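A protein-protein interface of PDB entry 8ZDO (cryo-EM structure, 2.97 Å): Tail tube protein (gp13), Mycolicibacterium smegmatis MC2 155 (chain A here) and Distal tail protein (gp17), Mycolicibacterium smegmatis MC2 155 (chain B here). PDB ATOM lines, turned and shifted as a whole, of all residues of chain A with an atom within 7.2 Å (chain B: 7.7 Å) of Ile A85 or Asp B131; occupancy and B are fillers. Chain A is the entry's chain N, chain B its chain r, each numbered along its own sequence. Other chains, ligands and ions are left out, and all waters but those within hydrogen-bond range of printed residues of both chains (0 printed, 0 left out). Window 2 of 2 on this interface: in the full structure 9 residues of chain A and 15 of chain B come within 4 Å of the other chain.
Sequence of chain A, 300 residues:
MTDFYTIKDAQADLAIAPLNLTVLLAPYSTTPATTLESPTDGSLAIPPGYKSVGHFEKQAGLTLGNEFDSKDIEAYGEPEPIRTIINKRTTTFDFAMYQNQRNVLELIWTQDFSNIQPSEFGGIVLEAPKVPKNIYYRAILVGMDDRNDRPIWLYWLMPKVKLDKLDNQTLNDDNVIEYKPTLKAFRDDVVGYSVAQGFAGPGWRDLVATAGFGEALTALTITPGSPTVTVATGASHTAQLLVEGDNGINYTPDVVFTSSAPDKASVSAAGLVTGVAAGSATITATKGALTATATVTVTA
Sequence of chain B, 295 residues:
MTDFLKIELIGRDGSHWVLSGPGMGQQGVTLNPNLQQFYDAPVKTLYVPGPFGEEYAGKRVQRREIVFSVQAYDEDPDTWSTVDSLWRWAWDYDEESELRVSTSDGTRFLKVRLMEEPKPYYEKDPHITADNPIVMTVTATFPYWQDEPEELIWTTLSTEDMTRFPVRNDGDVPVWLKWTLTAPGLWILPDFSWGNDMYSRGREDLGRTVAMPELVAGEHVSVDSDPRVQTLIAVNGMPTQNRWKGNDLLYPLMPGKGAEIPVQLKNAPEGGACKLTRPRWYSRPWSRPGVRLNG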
ATOM      1  N   ASP A  69      30.680 -26.896 -11.213  1.00  0.00           N
ATOM      2  CA  ASP A  69      30.345 -25.486 -11.337  1.00  0.00           C
ATOM      3  C   ASP A  69      28.830 -25.385 -11.444  1.00  0.00           C
ATOM      4  O   ASP A  69      28.235 -25.935 -12.375  1.00  0.00           O
ATOM      5  CB  ASP A  69      31.027 -24.864 -12.555  1.00  0.00           C
ATOM      6  CG  ASP A  69      30.938 -23.351 -12.564  1.00  0.00           C
ATOM      7  OD1 ASP A  69      30.497 -22.773 -11.550  1.00  0.00           O
ATOM      8  OD2 ASP A  69      31.312 -22.739 -13.587  1.00  0.00           O
ATOM      9  N   SER A  70      28.208 -24.709 -10.484  1.00  0.00           N
ATOM     10  CA  SER A  70      26.758 -24.676 -10.376  1.00  0.00           C
ATOM     11  C   SER A  70      26.254 -23.242 -10.394  1.00  0.00           C
ATOM     12  O   SER A  70      26.956 -22.310  -9.995  1.00  0.00           O
ATOM     13  CB  SER A  70      26.282 -25.375  -9.098  1.00  0.00           C
ATOM     14  OG  SER A  70      26.734 -26.716  -9.054  1.00  0.00           O
ATOM     15  N   LYS A  71      25.021 -23.082 -10.866  1.00  0.00           N
ATOM     16  CA  LYS A  71      24.371 -21.781 -10.950  1.00  0.00           C
ATOM     17  C   LYS A  71      22.939 -21.930 -10.466  1.00  0.00           C
ATOM     18  O   LYS A  71      22.178 -22.724 -11.023  1.00  0.00           O
ATOM     19  CB  LYS A  71      24.406 -21.245 -12.384  1.00  0.00           C
ATOM     20  CG  LYS A  71      23.543 -20.025 -12.617  1.00  0.00           C
ATOM     21  CD  LYS A  71      23.519 -19.651 -14.088  1.00  0.00           C
ATOM     22  CE  LYS A  71      24.926 -19.537 -14.652  1.00  0.00           C
ATOM     23  NZ  LYS A  71      24.923 -19.095 -16.072  1.00  0.00           N
ATOM     24  N   ASP A  72      22.575 -21.176  -9.433  1.00  0.00           N
ATOM     25  CA  ASP A  72      21.234 -21.261  -8.870  1.00  0.00           C
ATOM     26  C   ASP A  72      20.265 -20.411  -9.678  1.00  0.00           C
ATOM     27  O   ASP A  72      20.510 -19.223  -9.907  1.00  0.00           O
ATOM     28  CB  ASP A  72      21.236 -20.805  -7.412  1.00  0.00           C
ATOM     29  CG  ASP A  72      21.412 -21.955  -6.441  1.00  0.00           C
ATOM     30  OD1 ASP A  72      21.097 -23.103  -6.812  1.00  0.00           O
ATOM     31  OD2 ASP A  72      21.864 -21.707  -5.304  1.00  0.00           O
ATOM     32  N   ILE A  73      19.166 -21.020 -10.111  1.00  0.00           N
ATOM     33  CA  ILE A  73      18.077 -20.318 -10.768  1.00  0.00           C
ATOM     34  C   ILE A  73      16.991 -20.092  -9.730  1.00  0.00           C
ATOM     35  O   ILE A  73      16.411 -21.051  -9.204  1.00  0.00           O
ATOM     36  CB  ILE A  73      17.535 -21.108 -11.967  1.00  0.00           C
ATOM     37  CG1 ILE A  73      18.670 -21.466 -12.925  1.00  0.00           C
ATOM     38  CG2 ILE A  73      16.454 -20.314 -12.679  1.00  0.00           C
ATOM     39  CD1 ILE A  73      19.215 -20.287 -13.693  1.00  0.00           C
ATOM     40  N   ILE A  82      14.483 -21.997  -7.322  1.00  0.00           N
ATOM     41  CA  ILE A  82      13.614 -23.049  -7.837  1.00  0.00           C
ATOM     42  C   ILE A  82      14.438 -24.187  -8.421  1.00  0.00           C
ATOM     43  O   ILE A  82      14.076 -25.362  -8.290  1.00  0.00           O
ATOM     44  CB  ILE A  82      12.619 -22.481  -8.866  1.00  0.00           C
ATOM     45  CG1 ILE A  82      13.331 -21.590  -9.881  1.00  0.00           C
ATOM     46  CG2 ILE A  82      11.519 -21.707  -8.167  1.00  0.00           C
ATOM     47  CD1 ILE A  82      12.462 -21.204 -11.056  1.00  0.00           C
ATOM     48  N   ARG A  83      15.556 -23.868  -9.070  1.00  0.00           N
ATOM     49  CA  ARG A  83      16.365 -24.887  -9.722  1.00  0.00           C
ATOM     50  C   ARG A  83      17.841 -24.560  -9.556  1.00  0.00           C
ATOM     51  O   ARG A  83      18.219 -23.509  -9.038  1.00  0.00           O
ATOM     52  CB  ARG A  83      16.021 -25.005 -11.211  1.00  0.00           C
ATOM     53  CG  ARG A  83      14.910 -25.991 -11.517  1.00  0.00           C
ATOM     54  CD  ARG A  83      14.596 -26.017 -13.000  1.00  0.00           C
ATOM     55  NE  ARG A  83      13.707 -24.932 -13.392  1.00  0.00           N
ATOM     56  CZ  ARG A  83      14.102 -23.830 -14.011  1.00  0.00           C
ATOM     57  NH1 ARG A  83      15.373 -23.626 -14.310  1.00  0.00           N
ATOM     58  NH2 ARG A  83      13.201 -22.910 -14.340  1.00  0.00           N
ATOM     59  N   THR A  84      18.681 -25.483 -10.012  1.00  0.00           N
ATOM     60  CA  THR A  84      20.108 -25.230 -10.131  1.00  0.00           C
ATOM     61  C   THR A  84      20.630 -25.975 -11.349  1.00  0.00           C
ATOM     62  O   THR A  84      20.152 -27.063 -11.681  1.00  0.00           O
ATOM     63  CB  THR A  84      20.875 -25.639  -8.869  1.00  0.00           C
ATOM     64  OG1 THR A  84      22.279 -25.433  -9.072  1.00  0.00           O
ATOM     65  CG2 THR A  84      20.627 -27.091  -8.532  1.00  0.00           C
ATOM     66  N   ILE A  85      21.602 -25.370 -12.022  1.00  0.00           N
ATOM     67  CA  ILE A  85      22.173 -25.904 -13.252  1.00  0.00           C
ATOM     68  C   ILE A  85      23.639 -26.216 -13.006  1.00  0.00           C
ATOM     69  O   ILE A  85      24.386 -25.358 -12.525  1.00  0.00           O
ATOM     70  CB  ILE A  85      22.028 -24.917 -14.423  1.00  0.00           C
ATOM     71  CG1 ILE A  85      20.622 -24.323 -14.458  1.00  0.00           C
ATOM     72  CG2 ILE A  85      22.347 -25.603 -15.736  1.00  0.00           C
ATOM     73  CD1 ILE A  85      20.440 -23.298 -15.549  1.00  0.00           C
ATOM     74  N   ILE A  86      24.049 -27.434 -13.341  1.00  0.00           N
ATOM     75  CA  ILE A  86      25.457 -27.811 -13.322  1.00  0.00           C
ATOM     76  C   ILE A  86      26.017 -27.476 -14.700  1.00  0.00           C
ATOM     77  O   ILE A  86      25.806 -28.208 -15.666  1.00  0.00           O
ATOM     78  CB  ILE A  86      25.651 -29.286 -12.975  1.00  0.00           C
ATOM     79  CG1 ILE A  86      24.843 -29.652 -11.732  1.00  0.00           C
ATOM     80  CG2 ILE A  86      27.119 -29.584 -12.756  1.00  0.00           C
ATOM     81  CD1 ILE A  86      24.926 -31.112 -11.369  1.00  0.00           C
ATOM     82  N   ASN A  87      26.725 -26.348 -14.791  1.00  0.00           N
ATOM     83  CA  ASN A  87      27.291 -25.935 -16.069  1.00  0.00           C
ATOM     84  C   ASN A  87      28.339 -26.926 -16.555  1.00  0.00           C
ATOM     85  O   ASN A  87      28.376 -27.269 -17.743  1.00  0.00           O
ATOM     86  CB  ASN A  87      27.891 -24.536 -15.947  1.00  0.00           C
ATOM     87  CG  ASN A  87      26.872 -23.500 -15.531  1.00  0.00           C
ATOM     88  OD1 ASN A  87      27.012 -22.857 -14.493  1.00  0.00           O
ATOM     89  ND2 ASN A  87      25.836 -23.332 -16.344  1.00  0.00           N
ATOM     90  N   LYS A  88      29.196 -27.398 -15.654  1.00  0.00           N
ATOM     91  CA  LYS A  88      30.260 -28.314 -16.030  1.00  0.00           C
ATOM     92  C   LYS A  88      30.659 -29.150 -14.826  1.00  0.00           C
ATOM     93  O   LYS A  88      30.437 -28.767 -13.675  1.00  0.00           O
ATOM     94  CB  LYS A  88      31.477 -27.562 -16.580  1.00  0.00           C
ATOM     95  CG  LYS A  88      32.236 -26.772 -15.530  1.00  0.00           C
ATOM     96  CD  LYS A  88      33.364 -25.975 -16.153  1.00  0.00           C
ATOM     97  CE  LYS A  88      32.832 -24.770 -16.908  1.00  0.00           C
ATOM     98  NZ  LYS A  88      33.932 -23.948 -17.482  1.00  0.00           N
ATOM     99  N   GLY B  28       6.732 -23.193 -19.331  1.00  0.00           N
ATOM    100  CA  GLY B  28       8.165 -23.239 -19.497  1.00  0.00           C
ATOM    101  C   GLY B  28       8.895 -21.962 -19.148  1.00  0.00           C
ATOM    102  O   GLY B  28      10.123 -21.992 -19.008  1.00  0.00           O
ATOM    103  N   THR B  30       9.375 -18.713 -16.547  1.00  0.00           N
ATOM    104  CA  THR B  30       9.155 -18.115 -15.239  1.00  0.00           C
ATOM    105  C   THR B  30       9.716 -16.700 -15.228  1.00  0.00           C
ATOM    106  O   THR B  30      10.456 -16.298 -16.125  1.00  0.00           O
ATOM    107  CB  THR B  30       9.801 -18.947 -14.124  1.00  0.00           C
ATOM    108  OG1 THR B  30      11.202 -18.657 -14.060  1.00  0.00           O
ATOM    109  CG2 THR B  30       9.610 -20.428 -14.383  1.00  0.00           C
ATOM    110  N   ASN B  32      12.018 -13.741 -13.404  1.00  0.00           N
ATOM    111  CA  ASN B  32      13.171 -13.505 -12.555  1.00  0.00           C
ATOM    112  C   ASN B  32      12.969 -12.239 -11.732  1.00  0.00           C
ATOM    113  O   ASN B  32      12.212 -11.348 -12.129  1.00  0.00           O
ATOM    114  CB  ASN B  32      14.431 -13.367 -13.401  1.00  0.00           C
ATOM    115  CG  ASN B  32      14.851 -14.672 -14.035  1.00  0.00           C
ATOM    116  OD1 ASN B  32      14.579 -15.747 -13.507  1.00  0.00           O
ATOM    117  ND2 ASN B  32      15.516 -14.586 -15.179  1.00  0.00           N
ATOM    118  N   VAL B  70      13.063 -13.024 -17.857  1.00  0.00           N
ATOM    119  CA  VAL B  70      12.332 -14.275 -17.746  1.00  0.00           C
ATOM    120  C   VAL B  70      13.325 -15.404 -17.955  1.00  0.00           C
ATOM    121  O   VAL B  70      14.415 -15.211 -18.485  1.00  0.00           O
ATOM    122  CB  VAL B  70      11.166 -14.373 -18.747  1.00  0.00           C
ATOM    123  CG1 VAL B  70      10.072 -13.396 -18.373  1.00  0.00           C
ATOM    124  CG2 VAL B  70      11.656 -14.114 -20.154  1.00  0.00           C
ATOM    125  N   GLN B  71      12.945 -16.589 -17.504  1.00  0.00           N
ATOM    126  CA  GLN B  71      13.767 -17.779 -17.650  1.00  0.00           C
ATOM    127  C   GLN B  71      12.958 -18.832 -18.384  1.00  0.00           C
ATOM    128  O   GLN B  71      11.914 -19.270 -17.888  1.00  0.00           O
ATOM    129  CB  GLN B  71      14.230 -18.301 -16.290  1.00  0.00           C
ATOM    130  CG  GLN B  71      15.328 -19.337 -16.368  1.00  0.00           C
ATOM    131  CD  GLN B  71      16.707 -18.729 -16.271  1.00  0.00           C
ATOM    132  OE1 GLN B  71      16.862 -17.572 -15.887  1.00  0.00           O
ATOM    133  NE2 GLN B  71      17.721 -19.508 -16.618  1.00  0.00           N
ATOM    134  N   ALA B  72      13.428 -19.220 -19.564  1.00  0.00           N
ATOM    135  CA  ALA B  72      12.823 -20.297 -20.332  1.00  0.00           C
ATOM    136  C   ALA B  72      13.601 -21.575 -20.061  1.00  0.00           C
ATOM    137  O   ALA B  72      14.812 -21.629 -20.294  1.00  0.00           O
ATOM    138  CB  ALA B  72      12.817 -19.975 -21.824  1.00  0.00           C
ATOM    139  N   TYR B  73      12.906 -22.592 -19.562  1.00  0.00           N
ATOM    140  CA  TYR B  73      13.543 -23.811 -19.094  1.00  0.00           C
ATOM    141  C   TYR B  73      12.824 -25.018 -19.667  1.00  0.00           C
ATOM    142  O   TYR B  73      11.608 -24.995 -19.864  1.00  0.00           O
ATOM    143  CB  TYR B  73      13.537 -23.898 -17.561  1.00  0.00           C
ATOM    144  CG  TYR B  73      13.676 -25.305 -17.025  1.00  0.00           C
ATOM    145  CD1 TYR B  73      14.918 -25.914 -16.930  1.00  0.00           C
ATOM    146  CD2 TYR B  73      12.562 -26.026 -16.618  1.00  0.00           C
ATOM    147  CE1 TYR B  73      15.048 -27.198 -16.447  1.00  0.00           C
ATOM    148  CE2 TYR B  73      12.683 -27.311 -16.136  1.00  0.00           C
ATOM    149  CZ  TYR B  73      13.928 -27.892 -16.052  1.00  0.00           C
ATOM    150  OH  TYR B  73      14.053 -29.172 -15.568  1.00  0.00           O
ATOM    151  N   ASP B  74      13.590 -26.078 -19.919  1.00  0.00           N
ATOM    152  CA  ASP B  74      12.998 -27.373 -20.206  1.00  0.00           C
ATOM    153  C   ASP B  74      14.075 -28.444 -20.121  1.00  0.00           C
ATOM    154  O   ASP B  74      15.272 -28.148 -20.138  1.00  0.00           O
ATOM    155  CB  ASP B  74      12.318 -27.383 -21.571  1.00  0.00           C
ATOM    156  CG  ASP B  74      11.427 -28.571 -21.750  1.00  0.00           C
ATOM    157  OD1 ASP B  74      11.401 -29.444 -20.864  1.00  0.00           O
ATOM    158  OD2 ASP B  74      10.704 -28.603 -22.748  1.00  0.00           O
ATOM    159  N   GLU B  75      13.628 -29.699 -20.022  1.00  0.00           N
ATOM    160  CA  GLU B  75      14.564 -30.805 -19.842  1.00  0.00           C
ATOM    161  C   GLU B  75      15.362 -31.087 -21.111  1.00  0.00           C
ATOM    162  O   GLU B  75      16.546 -31.434 -21.036  1.00  0.00           O
ATOM    163  CB  GLU B  75      13.822 -32.064 -19.389  1.00  0.00           C
ATOM    164  CG  GLU B  75      13.350 -32.038 -17.939  1.00  0.00           C
ATOM    165  CD  GLU B  75      11.989 -31.393 -17.759  1.00  0.00           C
ATOM    166  OE1 GLU B  75      11.357 -31.029 -18.769  1.00  0.00           O
ATOM    167  OE2 GLU B  75      11.545 -31.250 -16.601  1.00  0.00           O
ATOM    168  N   ASP B  76      14.744 -30.946 -22.282  1.00  0.00           N
ATOM    169  CA  ASP B  76      15.461 -31.280 -23.499  1.00  0.00           C
ATOM    170  C   ASP B  76      15.638 -30.052 -24.386  1.00  0.00           C
ATOM    171  O   ASP B  76      14.759 -29.185 -24.441  1.00  0.00           O
ATOM    172  CB  ASP B  76      14.737 -32.378 -24.290  1.00  0.00           C
ATOM    173  CG  ASP B  76      13.263 -32.102 -24.449  1.00  0.00           C
ATOM    174  OD1 ASP B  76      12.753 -31.201 -23.750  1.00  0.00           O
ATOM    175  OD2 ASP B  76      12.615 -32.782 -25.271  1.00  0.00           O
ATOM    176  N   PRO B  77      16.773 -29.954 -25.081  1.00  0.00           N
ATOM    177  CA  PRO B  77      17.048 -28.752 -25.884  1.00  0.00           C
ATOM    178  C   PRO B  77      16.043 -28.491 -26.991  1.00  0.00           C
ATOM    179  O   PRO B  77      15.752 -27.325 -27.275  1.00  0.00           O
ATOM    180  CB  PRO B  77      18.445 -29.034 -26.451  1.00  0.00           C
ATOM    181  CG  PRO B  77      19.059 -29.960 -25.464  1.00  0.00           C
ATOM    182  CD  PRO B  77      17.941 -30.845 -25.012  1.00  0.00           C
ATOM    183  N   TRP B  80      12.908 -27.134 -25.416  1.00  0.00           N
ATOM    184  CA  TRP B  80      13.284 -25.822 -24.910  1.00  0.00           C
ATOM    185  C   TRP B  80      13.324 -24.796 -26.034  1.00  0.00           C
ATOM    186  O   TRP B  80      12.925 -23.642 -25.847  1.00  0.00           O
ATOM    187  CB  TRP B  80      14.639 -25.875 -24.211  1.00  0.00           C
ATOM    188  CG  TRP B  80      15.197 -24.507 -24.065  1.00  0.00           C
ATOM    189  CD1 TRP B  80      14.953 -23.634 -23.051  1.00  0.00           C
ATOM    190  CD2 TRP B  80      16.041 -23.822 -24.992  1.00  0.00           C
ATOM    191  NE1 TRP B  80      15.611 -22.454 -23.276  1.00  0.00           N
ATOM    192  CE2 TRP B  80      16.283 -22.544 -24.465  1.00  0.00           C
ATOM    193  CE3 TRP B  80      16.621 -24.168 -26.214  1.00  0.00           C
ATOM    194  CZ2 TRP B  80      17.081 -21.617 -25.112  1.00  0.00           C
ATOM    195  CZ3 TRP B  80      17.405 -23.246 -26.856  1.00  0.00           C
ATOM    196  CH2 TRP B  80      17.628 -21.985 -26.308  1.00  0.00           C
ATOM    197  N   TYR B 121      19.796 -15.427 -23.628  1.00  0.00           N
ATOM    198  CA  TYR B 121      20.771 -16.493 -23.425  1.00  0.00           C
ATOM    199  C   TYR B 121      21.995 -16.026 -22.647  1.00  0.00           C
ATOM    200  O   TYR B 121      22.162 -14.833 -22.384  1.00  0.00           O
ATOM    201  CB  TYR B 121      21.219 -17.086 -24.760  1.00  0.00           C
ATOM    202  CG  TYR B 121      20.076 -17.410 -25.684  1.00  0.00           C
ATOM    203  CD1 TYR B 121      19.162 -18.397 -25.377  1.00  0.00           C
ATOM    204  CD2 TYR B 121      19.970 -16.784 -26.916  1.00  0.00           C
ATOM    205  CE1 TYR B 121      18.128 -18.692 -26.232  1.00  0.00           C
ATOM    206  CE2 TYR B 121      18.948 -17.082 -27.780  1.00  0.00           C
ATOM    207  CZ  TYR B 121      18.030 -18.037 -27.435  1.00  0.00           C
ATOM    208  OH  TYR B 121      17.007 -18.341 -28.299  1.00  0.00           O
ATOM    209  N   TYR B 122      22.847 -16.977 -22.270  1.00  0.00           N
ATOM    210  CA  TYR B 122      24.122 -16.705 -21.622  1.00  0.00           C
ATOM    211  C   TYR B 122      25.189 -16.434 -22.681  1.00  0.00           C
ATOM    212  O   TYR B 122      24.884 -16.175 -23.849  1.00  0.00           O
ATOM    213  CB  TYR B 122      24.513 -17.866 -20.713  1.00  0.00           C
ATOM    214  CG  TYR B 122      23.600 -18.060 -19.528  1.00  0.00           C
ATOM    215  CD1 TYR B 122      23.426 -17.052 -18.592  1.00  0.00           C
ATOM    216  CD2 TYR B 122      22.923 -19.255 -19.337  1.00  0.00           C
ATOM    217  CE1 TYR B 122      22.597 -17.225 -17.504  1.00  0.00           C
ATOM    218  CE2 TYR B 122      22.092 -19.436 -18.252  1.00  0.00           C
ATOM    219  CZ  TYR B 122      21.933 -18.418 -17.340  1.00  0.00           C
ATOM    220  OH  TYR B 122      21.106 -18.590 -16.255  1.00  0.00           O
ATOM    221  N   ASP B 125      26.567 -21.535 -25.772  1.00  0.00           N
ATOM    222  CA  ASP B 125      25.497 -22.091 -26.586  1.00  0.00           C
ATOM    223  C   ASP B 125      24.269 -22.361 -25.726  1.00  0.00           C
ATOM    224  O   ASP B 125      24.378 -23.063 -24.708  1.00  0.00           O
ATOM    225  CB  ASP B 125      25.972 -23.376 -27.259  1.00  0.00           C
ATOM    226  CG  ASP B 125      24.934 -23.979 -28.177  1.00  0.00           C
ATOM    227  OD1 ASP B 125      24.143 -23.221 -28.767  1.00  0.00           O
ATOM    228  OD2 ASP B 125      24.911 -25.218 -28.315  1.00  0.00           O
ATOM    229  N   PRO B 126      23.100 -21.822 -26.076  1.00  0.00           N
ATOM    230  CA  PRO B 126      21.914 -22.031 -25.232  1.00  0.00           C
ATOM    231  C   PRO B 126      21.496 -23.482 -25.095  1.00  0.00           C
ATOM    232  O   PRO B 126      20.973 -23.869 -24.041  1.00  0.00           O
ATOM    233  CB  PRO B 126      20.842 -21.200 -25.944  1.00  0.00           C
ATOM    234  CG  PRO B 126      21.335 -21.026 -27.333  1.00  0.00           C
ATOM    235  CD  PRO B 126      22.813 -20.935 -27.213  1.00  0.00           C
ATOM    236  N   HIS B 127      21.712 -24.301 -26.125  1.00  0.00           N
ATOM    237  CA  HIS B 127      21.306 -25.698 -26.064  1.00  0.00           C
ATOM    238  C   HIS B 127      22.124 -26.499 -25.063  1.00  0.00           C
ATOM    239  O   HIS B 127      21.728 -27.618 -24.718  1.00  0.00           O
ATOM    240  CB  HIS B 127      21.411 -26.334 -27.448  1.00  0.00           C
ATOM    241  CG  HIS B 127      20.587 -25.650 -28.492  1.00  0.00           C
ATOM    242  ND1 HIS B 127      21.084 -24.643 -29.290  1.00  0.00           N
ATOM    243  CD2 HIS B 127      19.301 -25.831 -28.873  1.00  0.00           C
ATOM    244  CE1 HIS B 127      20.139 -24.229 -30.114  1.00  0.00           C
ATOM    245  NE2 HIS B 127      19.046 -24.933 -29.881  1.00  0.00           N
ATOM    246  N   ILE B 128      23.252 -25.962 -24.594  1.00  0.00           N
ATOM    247  CA  ILE B 128      24.026 -26.644 -23.560  1.00  0.00           C
ATOM    248  C   ILE B 128      23.195 -26.793 -22.294  1.00  0.00           C
ATOM    249  O   ILE B 128      23.080 -27.885 -21.727  1.00  0.00           O
ATOM    250  CB  ILE B 128      25.335 -25.886 -23.277  1.00  0.00           C
ATOM    251  CG1 ILE B 128      26.301 -26.002 -24.453  1.00  0.00           C
ATOM    252  CG2 ILE B 128      25.979 -26.398 -22.002  1.00  0.00           C
ATOM    253  CD1 ILE B 128      27.414 -24.989 -24.407  1.00  0.00           C
ATOM    254  N   THR B 129      22.595 -25.696 -21.839  1.00  0.00           N
ATOM    255  CA  THR B 129      21.842 -25.706 -20.595  1.00  0.00           C
ATOM    256  C   THR B 129      20.355 -25.948 -20.799  1.00  0.00           C
ATOM    257  O   THR B 129      19.708 -26.516 -19.913  1.00  0.00           O
ATOM    258  CB  THR B 129      22.039 -24.386 -19.845  1.00  0.00           C
ATOM    259  OG1 THR B 129      21.945 -23.294 -20.765  1.00  0.00           O
ATOM    260  CG2 THR B 129      23.394 -24.357 -19.166  1.00  0.00           C
ATOM    261  N   ALA B 130      19.796 -25.532 -21.939  1.00  0.00           N
ATOM    262  CA  ALA B 130      18.356 -25.602 -22.188  1.00  0.00           C
ATOM    263  C   ALA B 130      17.561 -24.902 -21.091  1.00  0.00           C
ATOM    264  O   ALA B 130      16.399 -25.236 -20.841  1.00  0.00           O
ATOM    265  CB  ALA B 130      17.884 -27.051 -22.350  1.00  0.00           C
ATOM    266  N   ASP B 131      18.189 -23.937 -20.424  1.00  0.00           N
ATOM    267  CA  ASP B 131      17.560 -23.181 -19.344  1.00  0.00           C
ATOM    268  C   ASP B 131      18.219 -21.806 -19.349  1.00  0.00           C
ATOM    269  O   ASP B 131      19.254 -21.611 -18.709  1.00  0.00           O
ATOM    270  CB  ASP B 131      17.738 -23.894 -18.012  1.00  0.00           C
ATOM    271  CG  ASP B 131      17.015 -23.208 -16.881  1.00  0.00           C
ATOM    272  OD1 ASP B 131      16.235 -22.273 -17.149  1.00  0.00           O
ATOM    273  OD2 ASP B 131      17.220 -23.610 -15.718  1.00  0.00           O
ATOM    274  N   ASN B 132      17.611 -20.864 -20.060  1.00  0.00           N
ATOM    275  CA  ASN B 132      18.297 -19.621 -20.370  1.00  0.00           C
ATOM    276  C   ASN B 132      17.426 -18.411 -20.071  1.00  0.00           C
ATOM    277  O   ASN B 132      16.197 -18.474 -20.180  1.00  0.00           O
ATOM    278  CB  ASN B 132      18.721 -19.594 -21.844  1.00  0.00           C
ATOM    279  CG  ASN B 132      19.765 -20.637 -22.162  1.00  0.00           C
ATOM    280  OD1 ASN B 132      20.922 -20.510 -21.770  1.00  0.00           O
ATOM    281  ND2 ASN B 132      19.362 -21.684 -22.868  1.00  0.00           N
ATOM    282  N   PRO B 133      18.045 -17.291 -19.694  1.00  0.00           N
ATOM    283  CA  PRO B 133      17.287 -16.075 -19.398  1.00  0.00           C
ATOM    284  C   PRO B 133      17.181 -15.140 -20.591  1.00  0.00           C
ATOM    285  O   PRO B 133      18.126 -14.942 -21.355  1.00  0.00           O
ATOM    286  CB  PRO B 133      18.120 -15.431 -18.283  1.00  0.00           C
ATOM    287  CG  PRO B 133      19.523 -15.830 -18.612  1.00  0.00           C
ATOM    288  CD  PRO B 133      19.476 -17.123 -19.396  1.00  0.00           C
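NH1 of Arg A83 lies within salt-bridge range of OD1 of Asp B131 (3.3 Å).
O of Pro B126 is in hydrogen-bond range of OG1 of Thr B129 (3.5 Å).
O of Ile A73 sits at hydrogen-bond distance from N of Ile A82, at 2.9 Å.
The backbone carbonyl oxygen (O) of Gly B28 is in hydrogen-bond range of the backbone NH (N) of Tyr B73, at 2.9 Å.
The backbone carbonyl oxygen of Lys A71 lies within hydrogen-bond range of the side-chain hydroxyl of Thr A84, 3.3 Å away.
The side-chain amide oxygen (OD1) of Asn B132 is in hydrogen-bond range of the side-chain hydroxyl (OG1) of Thr B129 (3.1 Å).
The side-chain hydroxyl (OH) of Tyr B73 sits at hydrogen-bond distance from the side-chain carboxylate (OE2) of Glu B75, 3.4 Å away.
Among the printed residues, pairs that only touch across the chains: Ile A85 with Asp B131 (3.2 Å), Lys A71 with Tyr B122 (3.3 Å), Ile A73 with Gln B71 (3.4 Å), Arg A83 with Tyr B73 (3.4 Å), Ile A73 with Tyr B122 (3.6 Å), Ile A85 with Thr B129 (3.8 Å), Ile A73 with Asp B131 (3.8 Å) and Asn A87 with Thr B129 (3.9 Å).
Hydrophobic or aromatic side chains of chain A that line the printed part of chain B: Ile A73 and Ile A85.
Of the 23 printed residues of chain B, 5 touch a printed residue of chain A.
Hydrophobic or aromatic side chains of chain B within 4 Å of the printed part of chain A: Tyr B73 and Tyr B122.
Along chain B the printed residues that touch a printed residue of chain A span positions 71 to 131.
Of chain B, only Thr B129 and Asp B131 come within 4 Å of Ile A85.
Asp B131 touches just these residues of chain A: Ile A73, Arg A83 and Ile A85.
Printed residues of chain A within 4 Å of Thr B129: Ile A85 (3.8 Å) and Asn A87 (3.9 Å).
Printed residues of chain A within 4 Å of Gln B71: Ile A73 (3.4 Å).
Of the printed residues of chain A, Tyr B122 touches Lys A71 (3.3 Å) and Ile A73 (3.6 Å).
Printed residues of chain B within 4 Å of Asn A87: Thr B129 (3.9 Å).
Of the printed residues of chain B, Ile A73 touches Gln B71, Tyr B122 and Asp B131.
The nearest printed residue of chain B that does not touch Ile A85 is Gln B71 (4.8 Å).
The nearest residue of chain A that does not touch Asp B131 is Thr A84 (6.0 Å).
The nearest printed residue of chain A that does not touch Gln B71 is Arg A83 (4.6 Å).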
